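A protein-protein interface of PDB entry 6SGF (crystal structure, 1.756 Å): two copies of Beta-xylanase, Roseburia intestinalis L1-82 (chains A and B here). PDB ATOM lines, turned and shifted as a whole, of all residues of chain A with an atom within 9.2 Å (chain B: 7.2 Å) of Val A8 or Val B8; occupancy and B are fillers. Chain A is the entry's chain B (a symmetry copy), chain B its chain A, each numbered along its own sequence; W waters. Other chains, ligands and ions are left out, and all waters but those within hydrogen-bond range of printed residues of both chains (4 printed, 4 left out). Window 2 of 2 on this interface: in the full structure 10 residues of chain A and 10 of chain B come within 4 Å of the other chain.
N of Gln B60 is in hydrogen-bond range of O of Ser B125 (2.9 Å). The side-chain amide oxygen (OE1) of Gln B13 is in hydrogen-bond range of the backbone NH (N) of Thr B10. OG1 of Thr A10 is in hydrogen-bond range of OD1 of Asp A12, at 2.8 Å. The backbone NH (N) of Val A124 is in hydrogen-bond range of the backbone carbonyl oxygen (O) of Gln A60 (2.8 Å). O of Ser A125 sits at hydrogen-bond distance from N of Gln A60, at 2.9 Å. O of Gln B60 is in hydrogen-bond range of N of Val B124.
Water W4 bridges the side-chain amino group of Lys A7 (2.5 Å) and the backbone NH of Lys B6 (3.2 Å). Water W3 lies within hydrogen-bond range of O of Lys A6 (2.5 Å) and O of Lys B6 (2.7 Å). Water W1 bridges NE2 of Gln A60 (2.6 Å) and OG1 of Thr B10 (3.4 Å). Water W2 lies within hydrogen-bond range of the side-chain hydroxyl of Thr B127 and the side-chain amide oxygen of Gln A13.
Val A8 touches its own counterpart, Val B8. Thr A10 touches Gln B60, and with the chains exchanged Gln A60 touches Thr B10. Thr A10 touches Ser B125, and with the chains exchanged Ser A125 touches Thr B10.
The side-chain hydroxyl of Thr A10 sits at hydrogen-bond distance from the side-chain amide oxygen of Gln B60 (3.3 Å). The side-chain amide nitrogen (NE2) of Gln B60 sits close to the side-chain carboxylate (OD1) of Asp A12 (3.4 Å). OG1 of Thr B10 sits at hydrogen-bond distance from OE1 of Gln A60, 3.4 Å away.
Of the 13 printed residues of chain B, 4 touch a printed residue of chain A. Hydrophobic or aromatic side chains of chain B that line the printed part of chain A: Val B8. Of the 25 printed residues of chain A, 5 touch a printed residue of chain B. Hydrophobic or aromatic side chains of chain A that line the printed part of chain B: Val A8. Among the printed residues, no Asp or Glu carboxylate lies within 4 Å of a Lys or Arg side-chain nitrogen of the other chain.
Thr A58 touches none of the printed residues of chain B. Printed residues of chain B within 4 Å of Gln A60: Thr B10 (3.4 Å). Of the printed residues of chain B, Ser A125 touches Thr B10 (3.95 Å). Thr A127 touches none of the printed residues of chain B. Phe B9 touches none of the printed residues of chain A. Of the printed residues of chain A, Thr B10 touches Gln A60 (3.4 Å) and Ser A125 (3.95 Å). Printed residues of chain A within 4 Å of Gln B60: Thr A10 (3.3 Å) and Asp A12 (3.4 Å). Printed residues of chain A within 4 Å of Ser B125: Thr A10 (3.9 Å). The nearest residue of chain A that does not touch Val B8 is Thr A10 (4.4 Å). The nearest printed residue of chain A that does not touch Ser B125 is Asp A12 (6.5 Å).
Among the printed residues, pairs that only touch across the chains: Val A8 with Val B8, Thr A10 with Ser B125 and Ser A125 with Thr B10.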
ATOM      1  N   GLY A   4     -24.216  33.455 -23.799  1.00  0.00           N
ATOM      2  CA  GLY A   4     -24.753  33.079 -25.091  1.00  0.00           C
ATOM      3  C   GLY A   4     -23.806  32.176 -25.857  1.00  0.00           C
ATOM      4  O   GLY A   4     -24.249  31.379 -26.666  1.00  0.00           O
ATOM      5  N   VAL A   5     -22.506  32.287 -25.574  1.00  0.00           N
ATOM      6  CA  VAL A   5     -21.522  31.445 -26.244  1.00  0.00           C
ATOM      7  C   VAL A   5     -21.692  30.024 -25.729  1.00  0.00           C
ATOM      8  O   VAL A   5     -21.940  29.814 -24.534  1.00  0.00           O
ATOM      9  CB  VAL A   5     -20.104  31.968 -25.969  1.00  0.00           C
ATOM     10  CG1 VAL A   5     -19.056  30.915 -26.281  1.00  0.00           C
ATOM     11  CG2 VAL A   5     -19.847  33.238 -26.774  1.00  0.00           C
ATOM     12  N   LYS A   6     -21.570  29.049 -26.617  1.00  0.00           N
ATOM     13  CA  LYS A   6     -21.723  27.642 -26.222  1.00  0.00           C
ATOM     14  C   LYS A   6     -20.461  26.864 -26.499  1.00  0.00           C
ATOM     15  O   LYS A   6     -19.954  26.934 -27.582  1.00  0.00           O
ATOM     16  CB  LYS A   6     -22.811  26.945 -27.010  1.00  0.00           C
ATOM     17  CG  LYS A   6     -24.209  27.389 -26.690  1.00  0.00           C
ATOM     18  CD  LYS A   6     -25.165  26.575 -27.432  1.00  0.00           C
ATOM     19  CE  LYS A   6     -26.569  26.741 -26.948  1.00  0.00           C
ATOM     20  NZ  LYS A   6     -27.071  28.084 -27.273  1.00  0.00           N
ATOM     21  N   LYS A   7     -19.943  26.235 -25.480  1.00  0.00           N
ATOM     22  CA  LYS A   7     -18.853  25.293 -25.622  1.00  0.00           C
ATOM     23  C   LYS A   7     -19.441  23.882 -25.580  1.00  0.00           C
ATOM     24  O   LYS A   7     -20.023  23.480 -24.567  1.00  0.00           O
ATOM     25  CB  LYS A   7     -17.832  25.508 -24.509  1.00  0.00           C
ATOM     26  CG  LYS A   7     -16.941  26.768 -24.628  1.00  0.00           C
ATOM     27  CD  LYS A   7     -16.405  27.024 -26.054  1.00  0.00           C
ATOM     28  CE  LYS A   7     -15.965  25.741 -26.824  1.00  0.00           C
ATOM     29  NZ  LYS A   7     -14.546  25.314 -26.682  1.00  0.00           N
ATOM     30  N   VAL A   8     -19.348  23.150 -26.685  1.00  0.00           N
ATOM     31  CA  VAL A   8     -19.996  21.845 -26.809  1.00  0.00           C
ATOM     32  C   VAL A   8     -18.920  20.787 -26.913  1.00  0.00           C
ATOM     33  O   VAL A   8     -18.034  20.893 -27.759  1.00  0.00           O
ATOM     34  CB  VAL A   8     -20.913  21.771 -28.044  1.00  0.00           C
ATOM     35  CG1 VAL A   8     -21.480  20.367 -28.192  1.00  0.00           C
ATOM     36  CG2 VAL A   8     -22.032  22.778 -27.997  1.00  0.00           C
ATOM     37  N   PHE A   9     -19.009  19.751 -26.098  1.00  0.00           N
ATOM     38  CA  PHE A   9     -18.100  18.618 -26.200  1.00  0.00           C
ATOM     39  C   PHE A   9     -18.892  17.356 -26.486  1.00  0.00           C
ATOM     40  O   PHE A   9     -19.677  16.906 -25.635  1.00  0.00           O
ATOM     41  CB  PHE A   9     -17.285  18.465 -24.918  1.00  0.00           C
ATOM     42  CG  PHE A   9     -16.611  19.718 -24.487  1.00  0.00           C
ATOM     43  CD1 PHE A   9     -15.624  20.287 -25.268  1.00  0.00           C
ATOM     44  CD2 PHE A   9     -16.983  20.347 -23.317  1.00  0.00           C
ATOM     45  CE1 PHE A   9     -14.996  21.468 -24.876  1.00  0.00           C
ATOM     46  CE2 PHE A   9     -16.363  21.529 -22.912  1.00  0.00           C
ATOM     47  CZ  PHE A   9     -15.361  22.087 -23.700  1.00  0.00           C
ATOM     48  N   THR A  10     -18.638  16.746 -27.642  1.00  0.00           N
ATOM     49  CA  THR A  10     -19.210  15.441 -27.914  1.00  0.00           C
ATOM     50  C   THR A  10     -18.446  14.377 -27.109  1.00  0.00           C
ATOM     51  O   THR A  10     -17.384  14.641 -26.540  1.00  0.00           O
ATOM     52  CB  THR A  10     -19.189  15.124 -29.408  1.00  0.00           C
ATOM     53  OG1 THR A  10     -17.863  15.174 -29.928  1.00  0.00           O
ATOM     54  CG2 THR A  10     -20.056  16.134 -30.199  1.00  0.00           C
ATOM     55  N   ALA A  11     -19.040  13.173 -27.027  1.00  0.00           N
ATOM     56  CA  ALA A  11     -18.506  12.104 -26.187  1.00  0.00           C
ATOM     57  C   ALA A  11     -17.039  11.811 -26.484  1.00  0.00           C
ATOM     58  O   ALA A  11     -16.237  11.635 -25.559  1.00  0.00           O
ATOM     59  CB  ALA A  11     -19.338  10.832 -26.339  1.00  0.00           C
ATOM     60  N   ASP A  12     -16.655  11.777 -27.762  1.00  0.00           N
ATOM     61  CA  ASP A  12     -15.268  11.425 -28.047  1.00  0.00           C
ATOM     62  C   ASP A  12     -14.270  12.474 -27.579  1.00  0.00           C
ATOM     63  O   ASP A  12     -13.067  12.189 -27.571  1.00  0.00           O
ATOM     64  CB  ASP A  12     -15.065  11.142 -29.543  1.00  0.00           C
ATOM     65  CG  ASP A  12     -15.060  12.380 -30.407  1.00  0.00           C
ATOM     66  OD1 ASP A  12     -15.790  13.349 -30.114  1.00  0.00           O
ATOM     67  OD2 ASP A  12     -14.362  12.348 -31.447  1.00  0.00           O
ATOM     68  N   GLN A  13     -14.724  13.645 -27.135  1.00  0.00           N
ATOM     69  CA  GLN A  13     -13.810  14.645 -26.593  1.00  0.00           C
ATOM     70  C   GLN A  13     -13.663  14.576 -25.076  1.00  0.00           C
ATOM     71  O   GLN A  13     -12.810  15.275 -24.528  1.00  0.00           O
ATOM     72  CB  GLN A  13     -14.278  16.048 -26.991  1.00  0.00           C
ATOM     73  CG  GLN A  13     -14.489  16.262 -28.462  1.00  0.00           C
ATOM     74  CD  GLN A  13     -14.971  17.672 -28.769  1.00  0.00           C
ATOM     75  OE1 GLN A  13     -16.165  17.947 -28.792  1.00  0.00           O
ATOM     76  NE2 GLN A  13     -14.031  18.575 -28.999  1.00  0.00           N
ATOM     77  N   LEU A  14     -14.429  13.724 -24.401  1.00  0.00           N
ATOM     78  CA  LEU A  14     -14.466  13.649 -22.952  1.00  0.00           C
ATOM     79  C   LEU A  14     -13.694  12.398 -22.546  1.00  0.00           C
ATOM     80  O   LEU A  14     -14.083  11.284 -22.900  1.00  0.00           O
ATOM     81  CB  LEU A  14     -15.916  13.616 -22.464  1.00  0.00           C
ATOM     82  CG  LEU A  14     -16.729  14.879 -22.757  1.00  0.00           C
ATOM     83  CD1 LEU A  14     -18.179  14.652 -22.399  1.00  0.00           C
ATOM     84  CD2 LEU A  14     -16.137  16.041 -21.958  1.00  0.00           C
ATOM     85  N   LEU A  45     -12.916  17.637 -18.628  1.00  0.00           N
ATOM     86  CA  LEU A  45     -13.148  18.499 -19.777  1.00  0.00           C
ATOM     87  C   LEU A  45     -11.823  18.779 -20.485  1.00  0.00           C
ATOM     88  O   LEU A  45     -10.773  18.812 -19.846  1.00  0.00           O
ATOM     89  CB  LEU A  45     -13.791  19.799 -19.334  1.00  0.00           C
ATOM     90  CG  LEU A  45     -15.171  19.722 -18.661  1.00  0.00           C
ATOM     91  CD1 LEU A  45     -15.605  21.171 -18.431  1.00  0.00           C
ATOM     92  CD2 LEU A  45     -16.141  18.918 -19.522  1.00  0.00           C
ATOM     93  N   PRO A  46     -11.836  18.979 -21.800  1.00  0.00           N
ATOM     94  CA  PRO A  46     -10.565  19.294 -22.486  1.00  0.00           C
ATOM     95  C   PRO A  46      -9.902  20.567 -21.964  1.00  0.00           C
ATOM     96  O   PRO A  46      -8.683  20.721 -22.100  1.00  0.00           O
ATOM     97  CB  PRO A  46     -10.978  19.428 -23.960  1.00  0.00           C
ATOM     98  CG  PRO A  46     -12.282  18.745 -24.066  1.00  0.00           C
ATOM     99  CD  PRO A  46     -12.961  18.892 -22.738  1.00  0.00           C
ATOM    100  N   GLU A  47     -10.666  21.483 -21.365  1.00  0.00           N
ATOM    101  CA  GLU A  47     -10.186  22.785 -20.896  1.00  0.00           C
ATOM    102  C   GLU A  47     -11.101  23.173 -19.766  1.00  0.00           C
ATOM    103  O   GLU A  47     -12.280  22.881 -19.856  1.00  0.00           O
ATOM    104  CB  GLU A  47     -10.296  23.775 -22.051  1.00  0.00           C
ATOM    105  CG  GLU A  47     -11.797  24.051 -22.396  1.00  0.00           C
ATOM    106  CD  GLU A  47     -12.118  23.648 -23.828  1.00  0.00           C
ATOM    107  OE1 GLU A  47     -11.694  22.519 -24.200  1.00  0.00           O
ATOM    108  OE2 GLU A  47     -12.717  24.451 -24.576  1.00  0.00           O
ATOM    109  N   ILE A  49     -13.391  25.636 -17.531  1.00  0.00           N
ATOM    110  CA  ILE A  49     -14.250  26.780 -17.762  1.00  0.00           C
ATOM    111  C   ILE A  49     -14.534  27.340 -16.382  1.00  0.00           C
ATOM    112  O   ILE A  49     -14.843  26.578 -15.459  1.00  0.00           O
ATOM    113  CB  ILE A  49     -15.557  26.355 -18.456  1.00  0.00           C
ATOM    114  CG1 ILE A  49     -15.233  25.571 -19.735  1.00  0.00           C
ATOM    115  CG2 ILE A  49     -16.433  27.526 -18.706  1.00  0.00           C
ATOM    116  CD1 ILE A  49     -16.372  24.688 -20.256  1.00  0.00           C
ATOM    117  N   THR A  58     -25.790  21.489 -20.182  1.00  0.00           N
ATOM    118  CA  THR A  58     -26.812  20.602 -20.713  1.00  0.00           C
ATOM    119  C   THR A  58     -26.186  19.275 -21.136  1.00  0.00           C
ATOM    120  O   THR A  58     -25.274  19.246 -21.966  1.00  0.00           O
ATOM    121  CB  THR A  58     -27.543  21.258 -21.881  1.00  0.00           C
ATOM    122  OG1 THR A  58     -28.163  22.460 -21.418  1.00  0.00           O
ATOM    123  CG2 THR A  58     -28.626  20.319 -22.423  1.00  0.00           C
ATOM    124  N   GLN A  60     -26.738  15.786 -22.998  1.00  0.00           N
ATOM    125  CA  GLN A  60     -27.545  15.061 -23.966  1.00  0.00           C
ATOM    126  C   GLN A  60     -27.262  13.570 -23.846  1.00  0.00           C
ATOM    127  O   GLN A  60     -26.095  13.145 -23.899  1.00  0.00           O
ATOM    128  CB  GLN A  60     -27.257  15.541 -25.388  1.00  0.00           C
ATOM    129  CG  GLN A  60     -28.127  14.875 -26.458  1.00  0.00           C
ATOM    130  CD  GLN A  60     -27.895  15.446 -27.869  1.00  0.00           C
ATOM    131  OE1 GLN A  60     -26.937  16.179 -28.125  1.00  0.00           O
ATOM    132  NE2 GLN A  60     -28.769  15.101 -28.770  1.00  0.00           N
ATOM    133  N   GLU A  93     -32.358  15.627 -23.130  1.00  0.00           N
ATOM    134  CA  GLU A  93     -31.474  16.723 -22.737  1.00  0.00           C
ATOM    135  C   GLU A  93     -31.902  17.220 -21.370  1.00  0.00           C
ATOM    136  O   GLU A  93     -33.083  17.527 -21.160  1.00  0.00           O
ATOM    137  CB  GLU A  93     -31.521  17.856 -23.777  1.00  0.00           C
ATOM    138  CG  GLU A  93     -31.009  17.380 -25.111  1.00  0.00           C
ATOM    139  CD  GLU A  93     -30.565  18.482 -26.045  1.00  0.00           C
ATOM    140  OE1 GLU A  93     -30.958  19.644 -25.838  1.00  0.00           O
ATOM    141  OE2 GLU A  93     -29.807  18.164 -26.996  1.00  0.00           O
ATOM    142  N   VAL A 124     -24.199  11.482 -25.095  1.00  0.00           N
ATOM    143  CA  VAL A 124     -23.984  12.026 -26.433  1.00  0.00           C
ATOM    144  C   VAL A 124     -23.091  13.248 -26.403  1.00  0.00           C
ATOM    145  O   VAL A 124     -22.138  13.360 -27.179  1.00  0.00           O
ATOM    146  CB  VAL A 124     -25.354  12.367 -27.075  1.00  0.00           C
ATOM    147  CG1 VAL A 124     -25.180  13.054 -28.434  1.00  0.00           C
ATOM    148  CG2 VAL A 124     -26.236  11.120 -27.125  1.00  0.00           C
ATOM    149  N   SER A 125     -23.395  14.204 -25.534  1.00  0.00           N
ATOM    150  CA  SER A 125     -22.647  15.444 -25.529  1.00  0.00           C
ATOM    151  C   SER A 125     -22.937  16.183 -24.239  1.00  0.00           C
ATOM    152  O   SER A 125     -23.944  15.924 -23.579  1.00  0.00           O
ATOM    153  CB  SER A 125     -23.023  16.318 -26.716  1.00  0.00           C
ATOM    154  OG  SER A 125     -24.352  16.787 -26.613  1.00  0.00           O
ATOM    155  N   VAL A 126     -22.058  17.127 -23.923  1.00  0.00           N
ATOM    156  CA  VAL A 126     -22.253  18.074 -22.831  1.00  0.00           C
ATOM    157  C   VAL A 126     -21.970  19.472 -23.360  1.00  0.00           C
ATOM    158  O   VAL A 126     -20.950  19.697 -24.017  1.00  0.00           O
ATOM    159  CB  VAL A 126     -21.350  17.759 -21.627  1.00  0.00           C
ATOM    160  CG1 VAL A 126     -21.656  18.754 -20.484  1.00  0.00           C
ATOM    161  CG2 VAL A 126     -21.555  16.303 -21.177  1.00  0.00           C
ATOM    162  N   THR A 127     -22.900  20.389 -23.111  1.00  0.00           N
ATOM    163  CA  THR A 127     -22.845  21.753 -23.621  1.00  0.00           C
ATOM    164  C   THR A 127     -22.797  22.749 -22.472  1.00  0.00           C
ATOM    165  O   THR A 127     -23.611  22.666 -21.556  1.00  0.00           O
ATOM    166  CB  THR A 127     -24.073  22.072 -24.478  1.00  0.00           C
ATOM    167  OG1 THR A 127     -24.070  21.266 -25.678  1.00  0.00           O
ATOM    168  CG2 THR A 127     -24.044  23.566 -24.820  1.00  0.00           C
ATOM    169  N   PHE A 128     -21.851  23.683 -22.527  1.00  0.00           N
ATOM    170  CA  PHE A 128     -21.738  24.778 -21.569  1.00  0.00           C
ATOM    171  C   PHE A 128     -22.170  26.063 -22.246  1.00  0.00           C
ATOM    172  O   PHE A 128     -21.537  26.490 -23.218  1.00  0.00           O
ATOM    173  CB  PHE A 128     -20.309  24.895 -21.078  1.00  0.00           C
ATOM    174  CG  PHE A 128     -19.860  23.680 -20.328  1.00  0.00           C
ATOM    175  CD1 PHE A 128     -19.454  22.552 -21.006  1.00  0.00           C
ATOM    176  CD2 PHE A 128     -19.898  23.664 -18.956  1.00  0.00           C
ATOM    177  CE1 PHE A 128     -19.070  21.425 -20.320  1.00  0.00           C
ATOM    178  CE2 PHE A 128     -19.497  22.533 -18.253  1.00  0.00           C
ATOM    179  CZ  PHE A 128     -19.103  21.409 -18.945  1.00  0.00           C
ATOM    180  N   GLU A 129     -23.268  26.646 -21.776  1.00  0.00           N
ATOM    181  CA  GLU A 129     -23.704  27.939 -22.277  1.00  0.00           C
ATOM    182  C   GLU A 129     -23.274  29.032 -21.308  1.00  0.00           C
ATOM    183  O   GLU A 129     -23.637  28.999 -20.124  1.00  0.00           O
ATOM    184  CB  GLU A 129     -25.202  28.018 -22.518  1.00  0.00           C
ATOM    185  CG  GLU A 129     -25.504  29.391 -23.135  1.00  0.00           C
ATOM    186  CD  GLU A 129     -26.784  29.425 -23.874  1.00  0.00           C
ATOM    187  OE1 GLU A 129     -27.415  28.350 -23.938  1.00  0.00           O
ATOM    188  OE2 GLU A 129     -27.166  30.515 -24.382  1.00  0.00           O
ATOM    189  N   LEU A 130     -22.534  30.004 -21.803  1.00  0.00           N
ATOM    190  CA  LEU A 130     -21.981  31.028 -20.933  1.00  0.00           C
ATOM    191  C   LEU A 130     -23.021  32.122 -20.708  1.00  0.00           C
ATOM    192  O   LEU A 130     -23.955  32.307 -21.487  1.00  0.00           O
ATOM    193  CB  LEU A 130     -20.713  31.615 -21.530  1.00  0.00           C
ATOM    194  CG  LEU A 130     -19.662  30.592 -21.982  1.00  0.00           C
ATOM    195  CD1 LEU A 130     -18.402  31.307 -22.400  1.00  0.00           C
ATOM    196  CD2 LEU A 130     -19.386  29.579 -20.870  1.00  0.00           C
ATOM    197  N   LYS B   6     -14.776  27.074 -31.732  1.00  0.00           N
ATOM    198  CA  LYS B   6     -15.515  25.991 -32.379  1.00  0.00           C
ATOM    199  C   LYS B   6     -17.007  26.118 -32.088  1.00  0.00           C
ATOM    200  O   LYS B   6     -17.420  26.110 -30.925  1.00  0.00           O
ATOM    201  CB  LYS B   6     -14.989  24.638 -31.913  1.00  0.00           C
ATOM    202  CG  LYS B   6     -13.695  24.219 -32.576  1.00  0.00           C
ATOM    203  CD  LYS B   6     -13.088  23.017 -31.878  1.00  0.00           C
ATOM    204  CE  LYS B   6     -11.683  22.704 -32.422  1.00  0.00           C
ATOM    205  NZ  LYS B   6     -11.256  21.288 -32.157  1.00  0.00           N
ATOM    206  N   LYS B   7     -17.808  26.241 -33.146  1.00  0.00           N
ATOM    207  CA  LYS B   7     -19.261  26.155 -33.059  1.00  0.00           C
ATOM    208  C   LYS B   7     -19.671  24.739 -33.454  1.00  0.00           C
ATOM    209  O   LYS B   7     -19.434  24.320 -34.592  1.00  0.00           O
ATOM    210  CB  LYS B   7     -19.938  27.177 -33.971  1.00  0.00           C
ATOM    211  CG  LYS B   7     -19.590  28.605 -33.705  1.00  0.00           C
ATOM    212  CD  LYS B   7     -20.484  29.492 -34.572  1.00  0.00           C
ATOM    213  CE  LYS B   7     -20.572  30.893 -34.033  1.00  0.00           C
ATOM    214  NZ  LYS B   7     -21.803  31.577 -34.521  1.00  0.00           N
ATOM    215  N   VAL B   8     -20.270  24.007 -32.519  1.00  0.00           N
ATOM    216  CA  VAL B   8     -20.595  22.598 -32.708  1.00  0.00           C
ATOM    217  C   VAL B   8     -22.112  22.451 -32.767  1.00  0.00           C
ATOM    218  O   VAL B   8     -22.828  22.960 -31.897  1.00  0.00           O
ATOM    219  CB  VAL B   8     -19.990  21.739 -31.584  1.00  0.00           C
ATOM    220  CG1 VAL B   8     -20.300  20.256 -31.784  1.00  0.00           C
ATOM    221  CG2 VAL B   8     -18.510  21.976 -31.479  1.00  0.00           C
ATOM    222  N   PHE B   9     -22.601  21.755 -33.793  1.00  0.00           N
ATOM    223  CA  PHE B   9     -24.018  21.403 -33.893  1.00  0.00           C
ATOM    224  C   PHE B   9     -24.147  19.892 -33.823  1.00  0.00           C
ATOM    225  O   PHE B   9     -23.671  19.179 -34.715  1.00  0.00           O
ATOM    226  CB  PHE B   9     -24.619  21.963 -35.188  1.00  0.00           C
ATOM    227  CG  PHE B   9     -24.407  23.451 -35.340  1.00  0.00           C
ATOM    228  CD1 PHE B   9     -24.917  24.328 -34.404  1.00  0.00           C
ATOM    229  CD2 PHE B   9     -23.677  23.959 -36.387  1.00  0.00           C
ATOM    230  CE1 PHE B   9     -24.692  25.696 -34.505  1.00  0.00           C
ATOM    231  CE2 PHE B   9     -23.467  25.337 -36.510  1.00  0.00           C
ATOM    232  CZ  PHE B   9     -23.979  26.197 -35.560  1.00  0.00           C
ATOM    233  N   THR B  10     -24.806  19.394 -32.786  1.00  0.00           N
ATOM    234  CA  THR B  10     -25.088  17.962 -32.802  1.00  0.00           C
ATOM    235  C   THR B  10     -26.269  17.675 -33.725  1.00  0.00           C
ATOM    236  O   THR B  10     -26.991  18.587 -34.156  1.00  0.00           O
ATOM    237  CB  THR B  10     -25.357  17.427 -31.398  1.00  0.00           C
ATOM    238  OG1 THR B  10     -26.474  18.115 -30.846  1.00  0.00           O
ATOM    239  CG2 THR B  10     -24.150  17.639 -30.467  1.00  0.00           C
ATOM    240  N   GLN B  13     -29.712  19.234 -33.594  1.00  0.00           N
ATOM    241  CA  GLN B  13     -29.856  20.652 -33.913  1.00  0.00           C
ATOM    242  C   GLN B  13     -29.952  20.927 -35.408  1.00  0.00           C
ATOM    243  O   GLN B  13     -30.058  22.096 -35.816  1.00  0.00           O
ATOM    244  CB  GLN B  13     -28.685  21.409 -33.347  1.00  0.00           C
ATOM    245  CG  GLN B  13     -28.594  21.301 -31.869  1.00  0.00           C
ATOM    246  CD  GLN B  13     -27.411  22.056 -31.349  1.00  0.00           C
ATOM    247  OE1 GLN B  13     -26.272  21.614 -31.478  1.00  0.00           O
ATOM    248  NE2 GLN B  13     -27.670  23.206 -30.741  1.00  0.00           N
ATOM    249  N   PRO B  46     -28.679  25.729 -37.632  1.00  0.00           N
ATOM    250  CA  PRO B  46     -29.463  26.647 -36.781  1.00  0.00           C
ATOM    251  C   PRO B  46     -29.180  28.126 -37.058  1.00  0.00           C
ATOM    252  O   PRO B  46     -29.966  28.984 -36.633  1.00  0.00           O
ATOM    253  CB  PRO B  46     -29.048  26.268 -35.348  1.00  0.00           C
ATOM    254  CG  PRO B  46     -28.149  25.106 -35.444  1.00  0.00           C
ATOM    255  CD  PRO B  46     -27.763  24.869 -36.860  1.00  0.00           C
ATOM    256  N   GLN B  60     -18.567  14.601 -38.009  1.00  0.00           N
ATOM    257  CA  GLN B  60     -18.360  13.401 -37.199  1.00  0.00           C
ATOM    258  C   GLN B  60     -19.441  12.382 -37.517  1.00  0.00           C
ATOM    259  O   GLN B  60     -20.633  12.702 -37.461  1.00  0.00           O
ATOM    260  CB  GLN B  60     -18.330  13.718 -35.703  1.00  0.00           C
ATOM    261  CG  GLN B  60     -18.046  12.475 -34.837  1.00  0.00           C
ATOM    262  CD  GLN B  60     -17.923  12.824 -33.358  1.00  0.00           C
ATOM    263  OE1 GLN B  60     -18.135  13.962 -32.958  1.00  0.00           O
ATOM    264  NE2 GLN B  60     -17.616  11.851 -32.552  1.00  0.00           N
ATOM    265  N   VAL B 124     -23.219  12.274 -36.450  1.00  0.00           N
ATOM    266  CA  VAL B 124     -23.131  12.623 -35.029  1.00  0.00           C
ATOM    267  C   VAL B 124     -23.177  14.131 -34.817  1.00  0.00           C
ATOM    268  O   VAL B 124     -23.976  14.633 -34.024  1.00  0.00           O
ATOM    269  CB  VAL B 124     -21.838  12.032 -34.420  1.00  0.00           C
ATOM    270  CG1 VAL B 124     -21.635  12.503 -32.976  1.00  0.00           C
ATOM    271  CG2 VAL B 124     -21.809  10.500 -34.504  1.00  0.00           C
ATOM    272  N   SER B 125     -22.352  14.893 -35.535  1.00  0.00           N
ATOM    273  CA  SER B 125     -22.209  16.314 -35.293  1.00  0.00           C
ATOM    274  C   SER B 125     -21.472  16.945 -36.470  1.00  0.00           C
ATOM    275  O   SER B 125     -20.801  16.258 -37.249  1.00  0.00           O
ATOM    276  CB  SER B 125     -21.442  16.580 -33.989  1.00  0.00           C
ATOM    277  OG  SER B 125     -20.068  16.208 -34.092  1.00  0.00           O
ATOM    278  N   VAL B 126     -21.593  18.268 -36.548  1.00  0.00           N
ATOM    279  CA  VAL B 126     -20.853  19.111 -37.484  1.00  0.00           C
ATOM    280  C   VAL B 126     -20.253  20.281 -36.715  1.00  0.00           C
ATOM    281  O   VAL B 126     -20.949  20.977 -35.948  1.00  0.00           O
ATOM    282  CB  VAL B 126     -21.735  19.597 -38.646  1.00  0.00           C
ATOM    283  CG1 VAL B 126     -20.888  20.415 -39.637  1.00  0.00           C
ATOM    284  CG2 VAL B 126     -22.447  18.397 -39.308  1.00  0.00           C
ATOM    285  N   THR B 127     -18.952  20.474 -36.889  1.00  0.00           N
ATOM    286  CA  THR B 127     -18.199  21.477 -36.141  1.00  0.00           C
ATOM    287  C   THR B 127     -17.618  22.504 -37.099  1.00  0.00           C
ATOM    288  O   THR B 127     -16.973  22.128 -38.074  1.00  0.00           O
ATOM    289  CB  THR B 127     -17.079  20.824 -35.348  1.00  0.00           C
ATOM    290  OG1 THR B 127     -17.638  19.932 -34.374  1.00  0.00           O
ATOM    291  CG2 THR B 127     -16.223  21.886 -34.656  1.00  0.00           C
ATOM    292  N   PHE B 128     -17.839  23.790 -36.801  1.00  0.00           N
ATOM    293  CA  PHE B 128     -17.295  24.924 -37.544  1.00  0.00           C
ATOM    294  C   PHE B 128     -16.158  25.508 -36.729  1.00  0.00           C
ATOM    295  O   PHE B 128     -16.379  26.047 -35.635  1.00  0.00           O
ATOM    296  CB  PHE B 128     -18.380  25.961 -37.836  1.00  0.00           C
ATOM    297  CG  PHE B 128     -19.341  25.488 -38.879  1.00  0.00           C
ATOM    298  CD1 PHE B 128     -20.358  24.625 -38.536  1.00  0.00           C
ATOM    299  CD2 PHE B 128     -19.178  25.831 -40.206  1.00  0.00           C
ATOM    300  CE1 PHE B 128     -21.221  24.122 -39.503  1.00  0.00           C
ATOM    301  CE2 PHE B 128     -20.048  25.334 -41.173  1.00  0.00           C
ATOM    302  CZ  PHE B 128     -21.042  24.454 -40.816  1.00  0.00           C
HETATM  303  O   HOH W   1     -27.997  15.072 -31.283  1.00  0.00           O
HETATM  304  O   HOH W   2     -16.169  19.214 -31.893  1.00  0.00           O
HETATM  305  O   HOH W   3     -18.391  27.997 -29.246  1.00  0.00           O
HETATM  306  O   HOH W   4     -14.143  26.793 -28.600  1.00  0.00           O
